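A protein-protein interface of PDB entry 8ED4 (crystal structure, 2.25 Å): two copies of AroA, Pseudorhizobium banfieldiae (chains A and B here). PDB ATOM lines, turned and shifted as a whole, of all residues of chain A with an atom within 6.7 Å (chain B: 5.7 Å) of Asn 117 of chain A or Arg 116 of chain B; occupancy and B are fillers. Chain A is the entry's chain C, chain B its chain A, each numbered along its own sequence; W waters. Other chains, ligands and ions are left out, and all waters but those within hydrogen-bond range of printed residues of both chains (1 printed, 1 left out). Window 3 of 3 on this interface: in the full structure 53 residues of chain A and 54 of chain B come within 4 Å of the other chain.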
ATOM      1  N   ARG A   4     -28.442  17.061  19.444  1.00  0.00           N
ATOM      2  CA  ARG A   4     -27.110  17.445  18.905  1.00  0.00           C
ATOM      3  C   ARG A   4     -26.961  16.976  17.452  1.00  0.00           C
ATOM      4  O   ARG A   4     -26.177  17.615  16.719  1.00  0.00           O
ATOM      5  CB  ARG A   4     -25.995  16.876  19.787  1.00  0.00           C
ATOM      6  CG  ARG A   4     -25.924  17.518  21.164  1.00  0.00           C
ATOM      7  CD  ARG A   4     -24.845  16.840  21.972  1.00  0.00           C
ATOM      8  NE  ARG A   4     -24.758  17.316  23.345  1.00  0.00           N
ATOM      9  CZ  ARG A   4     -25.622  17.028  24.312  1.00  0.00           C
ATOM     10  NH1 ARG A   4     -26.684  16.273  24.065  1.00  0.00           N
ATOM     11  NH2 ARG A   4     -25.429  17.504  25.533  1.00  0.00           N
ATOM     12  N   ASN A  74     -14.895  16.773  22.829  1.00  0.00           N
ATOM     13  CA  ASN A  74     -14.633  18.096  22.219  1.00  0.00           C
ATOM     14  C   ASN A  74     -13.271  18.071  21.506  1.00  0.00           C
ATOM     15  O   ASN A  74     -12.590  17.004  21.513  1.00  0.00           O
ATOM     16  CB  ASN A  74     -14.747  19.243  23.235  1.00  0.00           C
ATOM     17  CG  ASN A  74     -15.287  20.519  22.607  1.00  0.00           C
ATOM     18  OD1 ASN A  74     -15.148  20.713  21.399  1.00  0.00           O
ATOM     19  ND2 ASN A  74     -15.930  21.370  23.394  1.00  0.00           N
ATOM     20  N   SER A 111     -16.186  22.934  27.778  1.00  0.00           N
ATOM     21  CA  SER A 111     -14.820  23.457  27.500  1.00  0.00           C
ATOM     22  C   SER A 111     -14.858  24.466  26.339  1.00  0.00           C
ATOM     23  O   SER A 111     -15.788  24.438  25.530  1.00  0.00           O
ATOM     24  CB  SER A 111     -13.805  22.371  27.229  1.00  0.00           C
ATOM     25  OG  SER A 111     -13.692  21.476  28.324  1.00  0.00           O
ATOM     26  N   PHE A 112     -13.826  25.301  26.253  1.00  0.00           N
ATOM     27  CA  PHE A 112     -13.614  26.276  25.157  1.00  0.00           C
ATOM     28  C   PHE A 112     -13.073  25.572  23.905  1.00  0.00           C
ATOM     29  O   PHE A 112     -11.964  24.991  23.961  1.00  0.00           O
ATOM     30  CB  PHE A 112     -12.644  27.362  25.618  1.00  0.00           C
ATOM     31  CG  PHE A 112     -12.308  28.378  24.563  1.00  0.00           C
ATOM     32  CD1 PHE A 112     -13.236  29.343  24.202  1.00  0.00           C
ATOM     33  CD2 PHE A 112     -11.052  28.399  23.973  1.00  0.00           C
ATOM     34  CE1 PHE A 112     -12.910  30.318  23.274  1.00  0.00           C
ATOM     35  CE2 PHE A 112     -10.733  29.365  23.032  1.00  0.00           C
ATOM     36  CZ  PHE A 112     -11.666  30.316  22.679  1.00  0.00           C
ATOM     37  N   SER A 113     -13.812  25.660  22.795  1.00  0.00           N
ATOM     38  CA  SER A 113     -13.368  25.160  21.469  1.00  0.00           C
ATOM     39  C   SER A 113     -13.613  26.192  20.373  1.00  0.00           C
ATOM     40  O   SER A 113     -14.782  26.481  20.114  1.00  0.00           O
ATOM     41  CB  SER A 113     -14.042  23.862  21.099  1.00  0.00           C
ATOM     42  OG  SER A 113     -13.464  23.365  19.901  1.00  0.00           O
ATOM     43  N   GLU A 114     -12.545  26.636  19.707  1.00  0.00           N
ATOM     44  CA  GLU A 114     -12.624  27.433  18.453  1.00  0.00           C
ATOM     45  C   GLU A 114     -13.165  26.534  17.335  1.00  0.00           C
ATOM     46  O   GLU A 114     -14.077  26.987  16.619  1.00  0.00           O
ATOM     47  CB  GLU A 114     -11.262  28.015  18.054  1.00  0.00           C
ATOM     48  CG  GLU A 114     -10.755  29.107  18.983  1.00  0.00           C
ATOM     49  CD  GLU A 114      -9.239  29.293  18.968  1.00  0.00           C
ATOM     50  OE1 GLU A 114      -8.562  28.778  19.919  1.00  0.00           O
ATOM     51  OE2 GLU A 114      -8.726  29.933  18.010  1.00  0.00           O
ATOM     52  N   ALA A 115     -12.633  25.312  17.214  1.00  0.00           N
ATOM     53  CA  ALA A 115     -12.969  24.303  16.178  1.00  0.00           C
ATOM     54  C   ALA A 115     -14.433  23.839  16.261  1.00  0.00           C
ATOM     55  O   ALA A 115     -15.008  23.607  15.203  1.00  0.00           O
ATOM     56  CB  ALA A 115     -12.031  23.128  16.275  1.00  0.00           C
ATOM     57  N   ARG A 116     -15.029  23.688  17.446  1.00  0.00           N
ATOM     58  CA  ARG A 116     -16.424  23.167  17.546  1.00  0.00           C
ATOM     59  C   ARG A 116     -17.358  24.238  18.116  1.00  0.00           C
ATOM     60  O   ARG A 116     -18.546  23.946  18.275  1.00  0.00           O
ATOM     61  CB  ARG A 116     -16.426  21.829  18.301  1.00  0.00           C
ATOM     62  CG  ARG A 116     -15.476  20.810  17.676  1.00  0.00           C
ATOM     63  CD  ARG A 116     -15.495  19.432  18.311  1.00  0.00           C
ATOM     64  NE  ARG A 116     -16.873  19.016  18.534  1.00  0.00           N
ATOM     65  CZ  ARG A 116     -17.639  18.398  17.644  1.00  0.00           C
ATOM     66  NH1 ARG A 116     -17.157  18.064  16.452  1.00  0.00           N
ATOM     67  NH2 ARG A 116     -18.887  18.103  17.975  1.00  0.00           N
ATOM     68  N   ASN A 117     -16.824  25.430  18.388  1.00  0.00           N
ATOM     69  CA  ASN A 117     -17.567  26.681  18.714  1.00  0.00           C
ATOM     70  C   ASN A 117     -18.268  26.544  20.077  1.00  0.00           C
ATOM     71  O   ASN A 117     -19.391  27.093  20.234  1.00  0.00           O
ATOM     72  CB  ASN A 117     -18.465  27.096  17.539  1.00  0.00           C
ATOM     73  CG  ASN A 117     -17.647  27.384  16.294  1.00  0.00           C
ATOM     74  OD1 ASN A 117     -17.732  26.655  15.308  1.00  0.00           O
ATOM     75  ND2 ASN A 117     -16.779  28.384  16.357  1.00  0.00           N
ATOM     76  N   THR A 118     -17.600  25.926  21.055  1.00  0.00           N
ATOM     77  CA  THR A 118     -18.137  25.782  22.436  1.00  0.00           C
ATOM     78  C   THR A 118     -17.577  26.901  23.324  1.00  0.00           C
ATOM     79  O   THR A 118     -16.333  27.127  23.306  1.00  0.00           O
ATOM     80  CB  THR A 118     -17.853  24.408  23.057  1.00  0.00           C
ATOM     81  OG1 THR A 118     -16.446  24.145  23.009  1.00  0.00           O
ATOM     82  CG2 THR A 118     -18.635  23.305  22.382  1.00  0.00           C
ATOM     83  N   GLN A 119     -18.476  27.562  24.059  1.00  0.00           N
ATOM     84  CA  GLN A 119     -18.151  28.518  25.153  1.00  0.00           C
ATOM     85  C   GLN A 119     -17.271  29.638  24.587  1.00  0.00           C
ATOM     86  O   GLN A 119     -16.195  29.904  25.161  1.00  0.00           O
ATOM     87  CB  GLN A 119     -17.483  27.775  26.309  1.00  0.00           C
ATOM     88  CG  GLN A 119     -18.403  26.783  27.003  1.00  0.00           C
ATOM     89  CD  GLN A 119     -19.567  27.425  27.717  1.00  0.00           C
ATOM     90  OE1 GLN A 119     -19.483  28.562  28.191  1.00  0.00           O
ATOM     91  NE2 GLN A 119     -20.662  26.678  27.819  1.00  0.00           N
ATOM     92  N   GLN A 120     -17.734  30.258  23.497  1.00  0.00           N
ATOM     93  CA  GLN A 120     -17.107  31.447  22.863  1.00  0.00           C
ATOM     94  C   GLN A 120     -17.308  32.680  23.769  1.00  0.00           C
ATOM     95  O   GLN A 120     -16.603  33.651  23.557  1.00  0.00           O
ATOM     96  CB  GLN A 120     -17.665  31.665  21.449  1.00  0.00           C
ATOM     97  CG  GLN A 120     -17.427  30.493  20.498  1.00  0.00           C
ATOM     98  CD  GLN A 120     -16.010  30.341  19.979  1.00  0.00           C
ATOM     99  OE1 GLN A 120     -15.796  30.040  18.797  1.00  0.00           O
ATOM    100  NE2 GLN A 120     -15.016  30.530  20.837  1.00  0.00           N
ATOM    101  N   GLU A 732     -24.754  29.104  27.943  1.00  0.00           N
ATOM    102  CA  GLU A 732     -24.285  28.868  26.551  1.00  0.00           C
ATOM    103  C   GLU A 732     -24.190  27.349  26.327  1.00  0.00           C
ATOM    104  O   GLU A 732     -23.258  26.863  25.669  1.00  0.00           O
ATOM    105  CB  GLU A 732     -22.966  29.614  26.304  1.00  0.00           C
ATOM    106  CG  GLU A 732     -22.606  29.730  24.828  1.00  0.00           C
ATOM    107  CD  GLU A 732     -21.422  30.622  24.462  1.00  0.00           C
ATOM    108  OE1 GLU A 732     -21.339  31.762  24.997  1.00  0.00           O
ATOM    109  OE2 GLU A 732     -20.613  30.199  23.591  1.00  0.00           O
ATOM    110  N   ILE B   6     -11.758  21.189   9.390  1.00  0.00           N
ATOM    111  CA  ILE B   6     -12.884  20.462   8.742  1.00  0.00           C
ATOM    112  C   ILE B   6     -12.342  19.929   7.415  1.00  0.00           C
ATOM    113  O   ILE B   6     -12.374  20.681   6.422  1.00  0.00           O
ATOM    114  CB  ILE B   6     -14.126  21.354   8.555  1.00  0.00           C
ATOM    115  CG1 ILE B   6     -14.632  21.908   9.888  1.00  0.00           C
ATOM    116  CG2 ILE B   6     -15.216  20.597   7.815  1.00  0.00           C
ATOM    117  CD1 ILE B   6     -15.821  22.854   9.760  1.00  0.00           C
ATOM    118  N   TYR B  73     -20.878  25.851   4.396  1.00  0.00           N
ATOM    119  CA  TYR B  73     -21.656  24.697   4.924  1.00  0.00           C
ATOM    120  C   TYR B  73     -22.115  24.949   6.366  1.00  0.00           C
ATOM    121  O   TYR B  73     -21.313  25.432   7.199  1.00  0.00           O
ATOM    122  CB  TYR B  73     -20.854  23.397   4.851  1.00  0.00           C
ATOM    123  CG  TYR B  73     -21.527  22.287   5.616  1.00  0.00           C
ATOM    124  CD1 TYR B  73     -22.717  21.740   5.163  1.00  0.00           C
ATOM    125  CD2 TYR B  73     -21.027  21.854   6.835  1.00  0.00           C
ATOM    126  CE1 TYR B  73     -23.375  20.758   5.883  1.00  0.00           C
ATOM    127  CE2 TYR B  73     -21.673  20.875   7.573  1.00  0.00           C
ATOM    128  CZ  TYR B  73     -22.848  20.327   7.091  1.00  0.00           C
ATOM    129  OH  TYR B  73     -23.475  19.363   7.808  1.00  0.00           O
ATOM    130  N   ASN B  74     -23.367  24.600   6.670  1.00  0.00           N
ATOM    131  CA  ASN B  74     -23.849  24.600   8.074  1.00  0.00           C
ATOM    132  C   ASN B  74     -25.087  23.701   8.225  1.00  0.00           C
ATOM    133  O   ASN B  74     -25.524  23.094   7.219  1.00  0.00           O
ATOM    134  CB  ASN B  74     -24.121  26.033   8.550  1.00  0.00           C
ATOM    135  CG  ASN B  74     -23.816  26.265  10.016  1.00  0.00           C
ATOM    136  OD1 ASN B  74     -23.551  25.321  10.757  1.00  0.00           O
ATOM    137  ND2 ASN B  74     -23.860  27.518  10.442  1.00  0.00           N
ATOM    138  N   VAL B  75     -25.603  23.616   9.459  1.00  0.00           N
ATOM    139  CA  VAL B  75     -26.882  22.952   9.827  1.00  0.00           C
ATOM    140  C   VAL B  75     -27.779  23.989  10.506  1.00  0.00           C
ATOM    141  O   VAL B  75     -27.382  24.529  11.542  1.00  0.00           O
ATOM    142  CB  VAL B  75     -26.631  21.742  10.749  1.00  0.00           C
ATOM    143  CG1 VAL B  75     -27.940  21.090  11.177  1.00  0.00           C
ATOM    144  CG2 VAL B  75     -25.680  20.726  10.118  1.00  0.00           C
ATOM    145  N   SER B 113     -26.748  28.388  14.108  1.00  0.00           N
ATOM    146  CA  SER B 113     -26.840  26.909  14.244  1.00  0.00           C
ATOM    147  C   SER B 113     -26.696  26.447  15.713  1.00  0.00           C
ATOM    148  O   SER B 113     -25.558  26.473  16.234  1.00  0.00           O
ATOM    149  CB  SER B 113     -25.807  26.248  13.377  1.00  0.00           C
ATOM    150  OG  SER B 113     -25.864  24.841  13.533  1.00  0.00           O
ATOM    151  N   GLU B 114     -27.782  25.969  16.341  1.00  0.00           N
ATOM    152  CA  GLU B 114     -27.709  25.248  17.651  1.00  0.00           C
ATOM    153  C   GLU B 114     -26.817  24.007  17.513  1.00  0.00           C
ATOM    154  O   GLU B 114     -25.954  23.778  18.373  1.00  0.00           O
ATOM    155  CB  GLU B 114     -29.075  24.774  18.129  1.00  0.00           C
ATOM    156  CG  GLU B 114     -30.007  25.901  18.504  1.00  0.00           C
ATOM    157  CD  GLU B 114     -31.457  25.466  18.424  1.00  0.00           C
ATOM    158  OE1 GLU B 114     -31.836  24.598  19.238  1.00  0.00           O
ATOM    159  OE2 GLU B 114     -32.177  25.930  17.488  1.00  0.00           O
ATOM    160  N   ALA B 115     -27.010  23.243  16.445  1.00  0.00           N
ATOM    161  CA  ALA B 115     -26.321  21.958  16.226  1.00  0.00           C
ATOM    162  C   ALA B 115     -24.824  22.206  16.027  1.00  0.00           C
ATOM    163  O   ALA B 115     -24.048  21.444  16.576  1.00  0.00           O
ATOM    164  CB  ALA B 115     -26.946  21.245  15.053  1.00  0.00           C
ATOM    165  N   ARG B 116     -24.426  23.229  15.259  1.00  0.00           N
ATOM    166  CA  ARG B 116     -22.984  23.485  14.963  1.00  0.00           C
ATOM    167  C   ARG B 116     -22.452  24.672  15.791  1.00  0.00           C
ATOM    168  O   ARG B 116     -21.253  24.999  15.635  1.00  0.00           O
ATOM    169  CB  ARG B 116     -22.748  23.738  13.476  1.00  0.00           C
ATOM    170  CG  ARG B 116     -23.065  22.580  12.538  1.00  0.00           C
ATOM    171  CD  ARG B 116     -22.177  22.647  11.291  1.00  0.00           C
ATOM    172  NE  ARG B 116     -21.363  21.448  11.227  1.00  0.00           N
ATOM    173  CZ  ARG B 116     -20.075  21.365  10.922  1.00  0.00           C
ATOM    174  NH1 ARG B 116     -19.367  22.436  10.631  1.00  0.00           N
ATOM    175  NH2 ARG B 116     -19.487  20.175  10.898  1.00  0.00           N
ATOM    176  N   ASN B 117     -23.309  25.295  16.613  1.00  0.00           N
ATOM    177  CA  ASN B 117     -22.947  26.313  17.641  1.00  0.00           C
ATOM    178  C   ASN B 117     -22.376  27.576  16.995  1.00  0.00           C
ATOM    179  O   ASN B 117     -21.436  28.137  17.548  1.00  0.00           O
ATOM    180  CB  ASN B 117     -21.972  25.738  18.669  1.00  0.00           C
ATOM    181  CG  ASN B 117     -22.560  24.551  19.395  1.00  0.00           C
ATOM    182  OD1 ASN B 117     -21.900  23.519  19.501  1.00  0.00           O
ATOM    183  ND2 ASN B 117     -23.799  24.679  19.844  1.00  0.00           N
ATOM    184  N   THR B 118     -22.938  28.006  15.865  1.00  0.00           N
ATOM    185  CA  THR B 118     -22.547  29.258  15.166  1.00  0.00           C
ATOM    186  C   THR B 118     -23.504  30.371  15.587  1.00  0.00           C
ATOM    187  O   THR B 118     -24.738  30.126  15.665  1.00  0.00           O
ATOM    188  CB  THR B 118     -22.513  29.073  13.645  1.00  0.00           C
ATOM    189  OG1 THR B 118     -23.770  28.540  13.227  1.00  0.00           O
ATOM    190  CG2 THR B 118     -21.373  28.179  13.206  1.00  0.00           C
ATOM    191  N   GLN B 120     -24.273  32.042  18.344  1.00  0.00           N
ATOM    192  CA  GLN B 120     -25.116  31.856  19.554  1.00  0.00           C
ATOM    193  C   GLN B 120     -25.425  33.227  20.166  1.00  0.00           C
ATOM    194  O   GLN B 120     -26.426  33.314  20.908  1.00  0.00           O
ATOM    195  CB  GLN B 120     -24.461  30.900  20.554  1.00  0.00           C
ATOM    196  CG  GLN B 120     -24.375  29.462  20.046  1.00  0.00           C
ATOM    197  CD  GLN B 120     -25.628  28.622  20.230  1.00  0.00           C
ATOM    198  OE1 GLN B 120     -25.553  27.389  20.312  1.00  0.00           O
ATOM    199  NE2 GLN B 120     -26.791  29.260  20.308  1.00  0.00           N
ATOM    200  N   ASP B 734     -14.316  33.288  14.208  1.00  0.00           N
ATOM    201  CA  ASP B 734     -12.892  33.104  14.599  1.00  0.00           C
ATOM    202  C   ASP B 734     -11.993  33.452  13.411  1.00  0.00           C
ATOM    203  O   ASP B 734     -10.885  33.998  13.653  1.00  0.00           O
ATOM    204  CB  ASP B 734     -12.636  31.691  15.133  1.00  0.00           C
ATOM    205  CG  ASP B 734     -13.305  31.457  16.476  1.00  0.00           C
ATOM    206  OD1 ASP B 734     -13.539  32.452  17.184  1.00  0.00           O
ATOM    207  OD2 ASP B 734     -13.633  30.296  16.789  1.00  0.00           O
HETATM  208  O   HOH W   1     -23.013  25.983  22.517  1.00  0.00           O
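OD2 of Asp 734 of chain B lies close to OE1 of Gln 120 of chain A (3.0 Å).
The side-chain carboxylate (OD2) of Asp 734 of chain B lies close to the backbone carbonyl oxygen (O) of Glu 114 of chain A (3.3 Å).
The side-chain hydroxyl (OG) of Ser 113 of chain B is in hydrogen-bond range of the backbone NH (N) of Arg 116 of chain B.
The side-chain amide nitrogen (ND2) of Asn 117 of chain B is in hydrogen-bond range of the backbone carbonyl oxygen (O) of Glu 114 of chain B, at 2.8 Å.
The side-chain amide oxygen (OE1) of Gln 120 of chain B sits at hydrogen-bond distance from the side-chain amide nitrogen (ND2) of Asn 117 of chain B.
The side-chain hydroxyl (OG) of Ser 113 of chain A is in hydrogen-bond range of the backbone NH (N) of Arg 116 of chain A.
The backbone carbonyl oxygen of Glu 114 of chain A is in hydrogen-bond range of the side-chain amide nitrogen of Asn 117 of chain A (3.1 Å).
The backbone NH (N) of Gln 120 of chain A lies within hydrogen-bond range of the side-chain carboxylate (OE2) of Glu 732 of chain A, at 2.9 Å.
Among the printed residues, pairs that only touch across the chains: Arg 116 of chain A with Arg 116 of chain B (3.9 Å), Arg 116 of chain A with Asn 117 of chain B (3.6 Å), Asn 117 of chain A with Arg 116 of chain B (3.9 Å), Asn 117 of chain A with Asn 117 of chain B (3.1 Å) and Asn 117 of chain A with Asp 734 of chain B (3.7 Å).
Asn 117 of chain A touches just these residues of chain B: Arg 116, Asn 117 and Asp 734.
Printed residues of chain A within 4 Å of Asn 117 of chain B: Arg 116 and Asn 117.
Of the printed residues of chain B, Glu 114 of chain A touches Asp 734 (3.3 Å).
Ser 113 of chain B touches none of the printed residues of chain A.
Gln 119 of chain A touches none of the printed residues of chain B.
The nearest residue of chain B that does not touch Asn 117 of chain A is Thr 118 of chain B (4.5 Å).
The nearest residue of chain A that does not touch Arg 116 of chain B is Arg 4 of chain A (6.1 Å).
Of the 13 printed residues of chain A, 4 touch a printed residue of chain B.
Of the 12 printed residues of chain B, 3 touch a printed residue of chain A.
Among the printed residues, 7 pairs touch across the chains.
Among the printed residues, no Asp or Glu carboxylate lies within 4 Å of a Lys or Arg side-chain nitrogen of the other chain.
Arg 116 of chain A touches its own counterpart, Arg 116 of chain B.
Arg 116 of chain A touches Asn 117 of chain B, and with the chains exchanged Asn 117 of chain A touches Arg 116 of chain B.
Asn 117 of chain B touches its own counterpart, Asn 117 of chain A.
Water W1 bridges the side-chain amide nitrogen of Asn 117 of chain B (3.1 Å) and the backbone carbonyl oxygen of Glu 732 of chain A (3.3 Å).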
